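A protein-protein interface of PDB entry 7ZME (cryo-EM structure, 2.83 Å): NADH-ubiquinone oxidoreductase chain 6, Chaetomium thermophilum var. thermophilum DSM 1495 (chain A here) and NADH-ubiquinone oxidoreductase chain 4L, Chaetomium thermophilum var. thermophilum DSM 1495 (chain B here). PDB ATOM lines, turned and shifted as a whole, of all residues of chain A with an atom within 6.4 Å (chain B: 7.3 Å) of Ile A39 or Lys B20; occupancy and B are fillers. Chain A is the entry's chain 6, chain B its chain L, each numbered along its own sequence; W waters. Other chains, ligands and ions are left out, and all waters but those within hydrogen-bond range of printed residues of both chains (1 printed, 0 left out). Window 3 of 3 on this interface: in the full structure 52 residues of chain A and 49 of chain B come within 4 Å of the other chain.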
ATOM      1  N   GLY A  34      15.481  15.618  24.344  1.00  0.00           N
ATOM      2  CA  GLY A  34      16.269  14.703  23.537  1.00  0.00           C
ATOM      3  C   GLY A  34      16.860  15.364  22.308  1.00  0.00           C
ATOM      4  O   GLY A  34      18.011  15.113  21.950  1.00  0.00           O
ATOM      5  N   ILE A  35      16.079  16.214  21.644  1.00  0.00           N
ATOM      6  CA  ILE A  35      16.578  16.930  20.474  1.00  0.00           C
ATOM      7  C   ILE A  35      17.699  17.880  20.873  1.00  0.00           C
ATOM      8  O   ILE A  35      18.759  17.922  20.237  1.00  0.00           O
ATOM      9  CB  ILE A  35      15.431  17.678  19.776  1.00  0.00           C
ATOM     10  CG1 ILE A  35      14.365  16.694  19.302  1.00  0.00           C
ATOM     11  CG2 ILE A  35      15.959  18.498  18.615  1.00  0.00           C
ATOM     12  CD1 ILE A  35      12.985  17.294  19.232  1.00  0.00           C
ATOM     13  N   CYS A  36      17.485  18.647  21.946  1.00  0.00           N
ATOM     14  CA  CYS A  36      18.458  19.643  22.372  1.00  0.00           C
ATOM     15  C   CYS A  36      19.781  19.022  22.797  1.00  0.00           C
ATOM     16  O   CYS A  36      20.778  19.740  22.916  1.00  0.00           O
ATOM     17  CB  CYS A  36      17.883  20.478  23.513  1.00  0.00           C
ATOM     18  SG  CYS A  36      16.884  21.895  23.011  1.00  0.00           S
ATOM     19  N   VAL A  37      19.830  17.708  22.999  1.00  0.00           N
ATOM     20  CA  VAL A  37      21.118  17.023  23.317  1.00  0.00           C
ATOM     21  C   VAL A  37      22.026  17.029  22.082  1.00  0.00           C
ATOM     22  O   VAL A  37      23.245  17.144  22.250  1.00  0.00           O
ATOM     23  CB  VAL A  37      20.878  15.583  23.807  1.00  0.00           C
ATOM     24  CG1 VAL A  37      22.171  14.800  23.960  1.00  0.00           C
ATOM     25  CG2 VAL A  37      20.087  15.537  25.099  1.00  0.00           C
ATOM     26  N   ILE A  38      21.458  16.920  20.880  1.00  0.00           N
ATOM     27  CA  ILE A  38      22.301  16.781  19.658  1.00  0.00           C
ATOM     28  C   ILE A  38      22.439  18.102  18.908  1.00  0.00           C
ATOM     29  O   ILE A  38      23.463  18.272  18.234  1.00  0.00           O
ATOM     30  CB  ILE A  38      21.763  15.638  18.775  1.00  0.00           C
ATOM     31  CG1 ILE A  38      20.307  15.861  18.367  1.00  0.00           C
ATOM     32  CG2 ILE A  38      21.944  14.303  19.480  1.00  0.00           C
ATOM     33  CD1 ILE A  38      19.706  14.713  17.597  1.00  0.00           C
ATOM     34  N   ILE A  39      21.459  18.999  19.014  1.00  0.00           N
ATOM     35  CA  ILE A  39      21.496  20.261  18.219  1.00  0.00           C
ATOM     36  C   ILE A  39      22.300  21.340  18.949  1.00  0.00           C
ATOM     37  O   ILE A  39      22.709  22.301  18.285  1.00  0.00           O
ATOM     38  CB  ILE A  39      20.069  20.723  17.869  1.00  0.00           C
ATOM     39  CG1 ILE A  39      19.335  21.279  19.092  1.00  0.00           C
ATOM     40  CG2 ILE A  39      19.289  19.607  17.194  1.00  0.00           C
ATOM     41  CD1 ILE A  39      17.999  21.903  18.777  1.00  0.00           C
ATOM     42  N   SER A  40      22.507  21.204  20.258  1.00  0.00           N
ATOM     43  CA  SER A  40      23.191  22.259  21.050  1.00  0.00           C
ATOM     44  C   SER A  40      24.650  22.435  20.629  1.00  0.00           C
ATOM     45  O   SER A  40      25.335  21.420  20.466  1.00  0.00           O
ATOM     46  CB  SER A  40      23.081  22.009  22.524  1.00  0.00           C
ATOM     47  OG  SER A  40      21.783  22.330  22.998  1.00  0.00           O
ATOM     48  N   LYS A  41      25.089  23.680  20.439  1.00  0.00           N
ATOM     49  CA  LYS A  41      26.504  23.970  20.100  1.00  0.00           C
ATOM     50  C   LYS A  41      27.416  23.640  21.280  1.00  0.00           C
ATOM     51  O   LYS A  41      28.525  23.136  21.033  1.00  0.00           O
ATOM     52  CB  LYS A  41      26.670  25.427  19.662  1.00  0.00           C
ATOM     53  CG  LYS A  41      25.992  25.791  18.349  1.00  0.00           C
ATOM     54  CD  LYS A  41      26.217  27.231  17.943  1.00  0.00           C
ATOM     55  CE  LYS A  41      25.743  28.219  18.987  1.00  0.00           C
ATOM     56  NZ  LYS A  41      26.023  29.617  18.587  1.00  0.00           N
ATOM     57  N   ASN A  42      27.000  23.952  22.507  1.00  0.00           N
ATOM     58  CA  ASN A  42      27.884  23.726  23.679  1.00  0.00           C
ATOM     59  C   ASN A  42      27.727  22.281  24.169  1.00  0.00           C
ATOM     60  O   ASN A  42      26.585  21.862  24.407  1.00  0.00           O
ATOM     61  CB  ASN A  42      27.658  24.772  24.773  1.00  0.00           C
ATOM     62  CG  ASN A  42      28.595  24.623  25.950  1.00  0.00           C
ATOM     63  OD1 ASN A  42      28.159  24.468  27.084  1.00  0.00           O
ATOM     64  ND2 ASN A  42      29.885  24.668  25.688  1.00  0.00           N
ATOM     65  N   SER A  46      24.378  20.338  26.240  1.00  0.00           N
ATOM     66  CA  SER A  46      23.737  19.117  25.694  1.00  0.00           C
ATOM     67  C   SER A  46      23.812  17.970  26.706  1.00  0.00           C
ATOM     68  O   SER A  46      22.986  17.054  26.602  1.00  0.00           O
ATOM     69  CB  SER A  46      24.432  18.760  24.409  1.00  0.00           C
ATOM     70  OG  SER A  46      25.560  17.940  24.637  1.00  0.00           O
ATOM     71  N   SER A  97      34.465  24.010  19.973  1.00  0.00           N
ATOM     72  CA  SER A  97      33.235  23.234  19.670  1.00  0.00           C
ATOM     73  C   SER A  97      32.027  24.156  19.480  1.00  0.00           C
ATOM     74  O   SER A  97      31.212  23.868  18.600  1.00  0.00           O
ATOM     75  CB  SER A  97      32.977  22.199  20.737  1.00  0.00           C
ATOM     76  OG  SER A  97      32.674  22.812  21.976  1.00  0.00           O
ATOM     77  N   GLN A 100      32.399  25.515  16.308  1.00  0.00           N
ATOM     78  CA  GLN A 100      32.097  24.433  15.337  1.00  0.00           C
ATOM     79  C   GLN A 100      30.586  24.455  15.108  1.00  0.00           C
ATOM     80  O   GLN A 100      29.841  24.597  16.097  1.00  0.00           O
ATOM     81  CB  GLN A 100      32.600  23.094  15.881  1.00  0.00           C
ATOM     82  CG  GLN A 100      32.407  21.915  14.939  1.00  0.00           C
ATOM     83  CD  GLN A 100      32.748  20.614  15.622  1.00  0.00           C
ATOM     84  OE1 GLN A 100      32.711  20.508  16.845  1.00  0.00           O
ATOM     85  NE2 GLN A 100      33.087  19.608  14.832  1.00  0.00           N
ATOM     86  N   SER A 101      30.147  24.314  13.857  1.00  0.00           N
ATOM     87  CA  SER A 101      28.700  24.473  13.560  1.00  0.00           C
ATOM     88  C   SER A 101      28.081  23.194  13.003  1.00  0.00           C
ATOM     89  O   SER A 101      28.646  22.110  13.248  1.00  0.00           O
ATOM     90  CB  SER A 101      28.470  25.635  12.628  1.00  0.00           C
ATOM     91  N   ASN A 102      26.972  23.326  12.273  1.00  0.00           N
ATOM     92  CA  ASN A 102      26.328  22.198  11.618  1.00  0.00           C
ATOM     93  C   ASN A 102      25.606  22.678  10.369  1.00  0.00           C
ATOM     94  O   ASN A 102      24.947  23.723  10.383  1.00  0.00           O
ATOM     95  CB  ASN A 102      25.341  21.504  12.563  1.00  0.00           C
ATOM     96  CG  ASN A 102      24.330  22.465  13.157  1.00  0.00           C
ATOM     97  OD1 ASN A 102      24.691  23.398  13.875  1.00  0.00           O
ATOM     98  ND2 ASN A 102      23.055  22.245  12.857  1.00  0.00           N
ATOM     99  N   LEU B  17      24.172  11.288  12.147  1.00  0.00           N
ATOM    100  CA  LEU B  17      24.291  12.656  11.574  1.00  0.00           C
ATOM    101  C   LEU B  17      25.030  13.547  12.562  1.00  0.00           C
ATOM    102  O   LEU B  17      24.743  14.749  12.588  1.00  0.00           O
ATOM    103  CB  LEU B  17      22.906  13.234  11.245  1.00  0.00           C
ATOM    104  CG  LEU B  17      22.193  12.669  10.017  1.00  0.00           C
ATOM    105  CD1 LEU B  17      23.153  12.499   8.850  1.00  0.00           C
ATOM    106  CD2 LEU B  17      21.501  11.356  10.337  1.00  0.00           C
ATOM    107  N   ASN B  18      25.976  12.974  13.307  1.00  0.00           N
ATOM    108  CA  ASN B  18      26.778  13.768  14.277  1.00  0.00           C
ATOM    109  C   ASN B  18      28.005  14.354  13.579  1.00  0.00           C
ATOM    110  O   ASN B  18      28.751  13.585  12.964  1.00  0.00           O
ATOM    111  CB  ASN B  18      27.225  12.940  15.487  1.00  0.00           C
ATOM    112  CG  ASN B  18      27.694  13.810  16.633  1.00  0.00           C
ATOM    113  OD1 ASN B  18      27.255  14.947  16.776  1.00  0.00           O
ATOM    114  ND2 ASN B  18      28.584  13.288  17.455  1.00  0.00           N
ATOM    115  N   ARG B  19      28.206  15.664  13.677  1.00  0.00           N
ATOM    116  CA  ARG B  19      29.398  16.316  13.082  1.00  0.00           C
ATOM    117  C   ARG B  19      30.081  17.123  14.187  1.00  0.00           C
ATOM    118  O   ARG B  19      30.701  18.152  13.861  1.00  0.00           O
ATOM    119  CB  ARG B  19      28.999  17.251  11.938  1.00  0.00           C
ATOM    120  CG  ARG B  19      28.615  16.557  10.639  1.00  0.00           C
ATOM    121  CD  ARG B  19      27.150  16.163  10.581  1.00  0.00           C
ATOM    122  NE  ARG B  19      26.754  15.516   9.338  1.00  0.00           N
ATOM    123  CZ  ARG B  19      26.863  14.215   9.095  1.00  0.00           C
ATOM    124  NH1 ARG B  19      26.468  13.725   7.933  1.00  0.00           N
ATOM    125  NH2 ARG B  19      27.377  13.411  10.007  1.00  0.00           N
ATOM    126  N   LYS B  20      29.952  16.682  15.442  1.00  0.00           N
ATOM    127  CA  LYS B  20      30.492  17.473  16.573  1.00  0.00           C
ATOM    128  C   LYS B  20      31.686  16.782  17.237  1.00  0.00           C
ATOM    129  O   LYS B  20      32.818  17.259  17.050  1.00  0.00           O
ATOM    130  CB  LYS B  20      29.360  17.740  17.567  1.00  0.00           C
ATOM    131  CG  LYS B  20      28.300  18.714  17.069  1.00  0.00           C
ATOM    132  CD  LYS B  20      27.514  19.377  18.177  1.00  0.00           C
ATOM    133  CE  LYS B  20      26.702  20.560  17.695  1.00  0.00           C
ATOM    134  NZ  LYS B  20      25.563  20.144  16.844  1.00  0.00           N
ATOM    135  N   ASN B  21      31.441  15.718  17.997  1.00  0.00           N
ATOM    136  CA  ASN B  21      32.523  15.030  18.747  1.00  0.00           C
ATOM    137  C   ASN B  21      32.110  13.581  18.998  1.00  0.00           C
ATOM    138  O   ASN B  21      30.920  13.281  18.871  1.00  0.00           O
ATOM    139  CB  ASN B  21      32.896  15.759  20.042  1.00  0.00           C
ATOM    140  CG  ASN B  21      31.703  16.192  20.863  1.00  0.00           C
ATOM    141  OD1 ASN B  21      31.003  15.362  21.433  1.00  0.00           O
ATOM    142  ND2 ASN B  21      31.475  17.490  20.946  1.00  0.00           N
ATOM    143  N   ILE B  22      33.066  12.728  19.344  1.00  0.00           N
ATOM    144  CA  ILE B  22      32.788  11.285  19.570  1.00  0.00           C
ATOM    145  C   ILE B  22      32.104  11.101  20.932  1.00  0.00           C
ATOM    146  O   ILE B  22      31.442  10.066  21.117  1.00  0.00           O
ATOM    147  CB  ILE B  22      34.111  10.507  19.435  1.00  0.00           C
ATOM    148  CG1 ILE B  22      34.845  10.883  18.147  1.00  0.00           C
ATOM    149  CG2 ILE B  22      33.899   9.008  19.550  1.00  0.00           C
ATOM    150  CD1 ILE B  22      36.331  10.636  18.196  1.00  0.00           C
ATOM    151  N   ILE B  23      32.249  12.048  21.859  1.00  0.00           N
ATOM    152  CA  ILE B  23      31.491  11.945  23.144  1.00  0.00           C
ATOM    153  C   ILE B  23      29.980  12.033  22.873  1.00  0.00           C
ATOM    154  O   ILE B  23      29.238  11.268  23.495  1.00  0.00           O
ATOM    155  CB  ILE B  23      32.005  12.937  24.212  1.00  0.00           C
ATOM    156  CG1 ILE B  23      33.289  12.429  24.868  1.00  0.00           C
ATOM    157  CG2 ILE B  23      30.943  13.212  25.263  1.00  0.00           C
ATOM    158  CD1 ILE B  23      33.702  13.196  26.101  1.00  0.00           C
ATOM    159  N   LEU B  24      29.550  12.906  21.965  1.00  0.00           N
ATOM    160  CA  LEU B  24      28.116  12.982  21.576  1.00  0.00           C
ATOM    161  C   LEU B  24      27.685  11.679  20.903  1.00  0.00           C
ATOM    162  O   LEU B  24      26.532  11.283  21.116  1.00  0.00           O
ATOM    163  CB  LEU B  24      27.857  14.192  20.676  1.00  0.00           C
ATOM    164  CG  LEU B  24      26.408  14.670  20.630  1.00  0.00           C
ATOM    165  CD1 LEU B  24      25.839  14.794  22.032  1.00  0.00           C
ATOM    166  CD2 LEU B  24      26.292  15.990  19.890  1.00  0.00           C
ATOM    167  N   MET B  25      28.551  11.058  20.101  1.00  0.00           N
ATOM    168  CA  MET B  25      28.142   9.746  19.532  1.00  0.00           C
ATOM    169  C   MET B  25      27.919   8.734  20.665  1.00  0.00           C
ATOM    170  O   MET B  25      26.925   8.001  20.581  1.00  0.00           O
ATOM    171  CB  MET B  25      29.196   9.234  18.545  1.00  0.00           C
ATOM    172  CG  MET B  25      29.303  10.068  17.291  1.00  0.00           C
ATOM    173  SD  MET B  25      30.566   9.463  16.150  1.00  0.00           S
ATOM    174  CE  MET B  25      29.671   8.154  15.319  1.00  0.00           C
ATOM    175  N   SER B  83      42.622  15.359  19.625  1.00  0.00           N
ATOM    176  CA  SER B  83      41.293  15.953  19.361  1.00  0.00           C
ATOM    177  C   SER B  83      40.298  14.806  19.262  1.00  0.00           C
ATOM    178  O   SER B  83      40.706  13.734  18.781  1.00  0.00           O
ATOM    179  CB  SER B  83      41.312  16.731  18.078  1.00  0.00           C
ATOM    180  OG  SER B  83      39.999  17.012  17.628  1.00  0.00           O
ATOM    181  N   ILE B  84      39.106  14.937  19.844  1.00  0.00           N
ATOM    182  CA  ILE B  84      38.081  13.868  19.663  1.00  0.00           C
ATOM    183  C   ILE B  84      36.934  14.512  18.904  1.00  0.00           C
ATOM    184  O   ILE B  84      35.781  14.117  19.104  1.00  0.00           O
ATOM    185  CB  ILE B  84      37.636  13.221  20.986  1.00  0.00           C
ATOM    186  CG1 ILE B  84      37.006  14.226  21.952  1.00  0.00           C
ATOM    187  CG2 ILE B  84      38.775  12.451  21.633  1.00  0.00           C
ATOM    188  CD1 ILE B  84      35.798  13.687  22.670  1.00  0.00           C
ATOM    189  N   ALA B  85      37.276  15.445  18.027  1.00  0.00           N
ATOM    190  CA  ALA B  85      36.250  16.162  17.254  1.00  0.00           C
ATOM    191  C   ALA B  85      36.152  15.494  15.889  1.00  0.00           C
ATOM    192  O   ALA B  85      37.177  15.443  15.185  1.00  0.00           O
ATOM    193  CB  ALA B  85      36.696  17.584  17.114  1.00  0.00           C
ATOM    194  N   ILE B  86      34.984  14.973  15.533  1.00  0.00           N
ATOM    195  CA  ILE B  86      34.830  14.412  14.172  1.00  0.00           C
ATOM    196  C   ILE B  86      34.950  15.590  13.209  1.00  0.00           C
ATOM    197  O   ILE B  86      34.374  16.653  13.517  1.00  0.00           O
ATOM    198  CB  ILE B  86      33.507  13.637  14.061  1.00  0.00           C
ATOM    199  CG1 ILE B  86      32.321  14.407  14.637  1.00  0.00           C
ATOM    200  CG2 ILE B  86      33.636  12.276  14.727  1.00  0.00           C
ATOM    201  CD1 ILE B  86      31.262  13.503  15.226  1.00  0.00           C
ATOM    202  N   GLU B  87      35.668  15.428  12.091  1.00  0.00           N
ATOM    203  CA  GLU B  87      35.925  16.606  11.220  1.00  0.00           C
ATOM    204  C   GLU B  87      35.467  16.379   9.781  1.00  0.00           C
ATOM    205  O   GLU B  87      35.749  15.293   9.237  1.00  0.00           O
ATOM    206  CB  GLU B  87      37.410  16.976  11.252  1.00  0.00           C
ATOM    207  CG  GLU B  87      37.878  17.476  12.606  1.00  0.00           C
ATOM    208  CD  GLU B  87      39.377  17.677  12.734  1.00  0.00           C
ATOM    209  OE1 GLU B  87      40.070  17.633  11.698  1.00  0.00           O
ATOM    210  OE2 GLU B  87      39.849  17.871  13.872  1.00  0.00           O
HETATM  211  O   HOH W   1      30.921  20.318  18.967  1.00  0.00           O
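Among the printed residues, pairs that only touch across the chains: Val A37 with Leu B24 (3.5 Å), Ile A38 with Leu B24 (3.99 Å), Ile A39 with Lys B20 (3.9 Å) and Ser A40 with Lys B20 (3.2 Å).
Of the printed residues of chain B, Val A37 touches Leu B24. Of chain A, only Ile A38, Ile A39, Ser A40 and Gln A100 come within 4 Å of Lys B20. Of the printed residues of chain A, Leu B24 touches Val A37 (3.5 Å) and Ile A38 (3.99 Å). Of the printed residues of chain A, Ile B86 touches Gln A100. The nearest residue of chain A that does not touch Lys B20 is Lys A41 (4.2 Å).
The backbone carbonyl oxygen (O) of Ile A38 sits at hydrogen-bond distance from the side-chain amino group (NZ) of Lys B20, 3.1 Å away. The side-chain amide nitrogen (NE2) of Gln A100 sits at hydrogen-bond distance from the backbone carbonyl oxygen (O) of Ile B86. NE2 of Gln A100 is in hydrogen-bond range of O of Lys B20 (3.2 Å). The backbone carbonyl oxygen (O) of Arg B19 sits at hydrogen-bond distance from the side-chain amide nitrogen (NE2) of Gln A100, at 3.0 Å.
Water W1 lies within hydrogen-bond range of OE1 of Gln A100 (2.8 Å) and ND2 of Asn B21 (3.5 Å).
Of the 14 printed residues of chain B, 4 touch a printed residue of chain A. Hydrophobic or aromatic side chains of chain B that line the printed part of chain A: Leu B24. Along chain B the printed residues that touch a printed residue of chain A span positions 19 to 86. Among the printed residues, 8 pairs touch across the chains.
The backbone carbonyl oxygen (O) of Lys B20 is in hydrogen-bond range of the backbone NH (N) of Ile B86 (3.5 Å). The backbone carbonyl oxygen of Cys A36 lies within hydrogen-bond range of the side-chain hydroxyl of Ser A40 (2.8 Å). N of Leu B24 lies within hydrogen-bond range of OD1 of Asn B21 (2.9 Å). O of Val A37 sits close to OG of Ser A46, 3.4 Å away. The side-chain amide oxygen (OD1) of Asn B18 sits at hydrogen-bond distance from the backbone NH (N) of Lys B20, at 3.5 Å.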
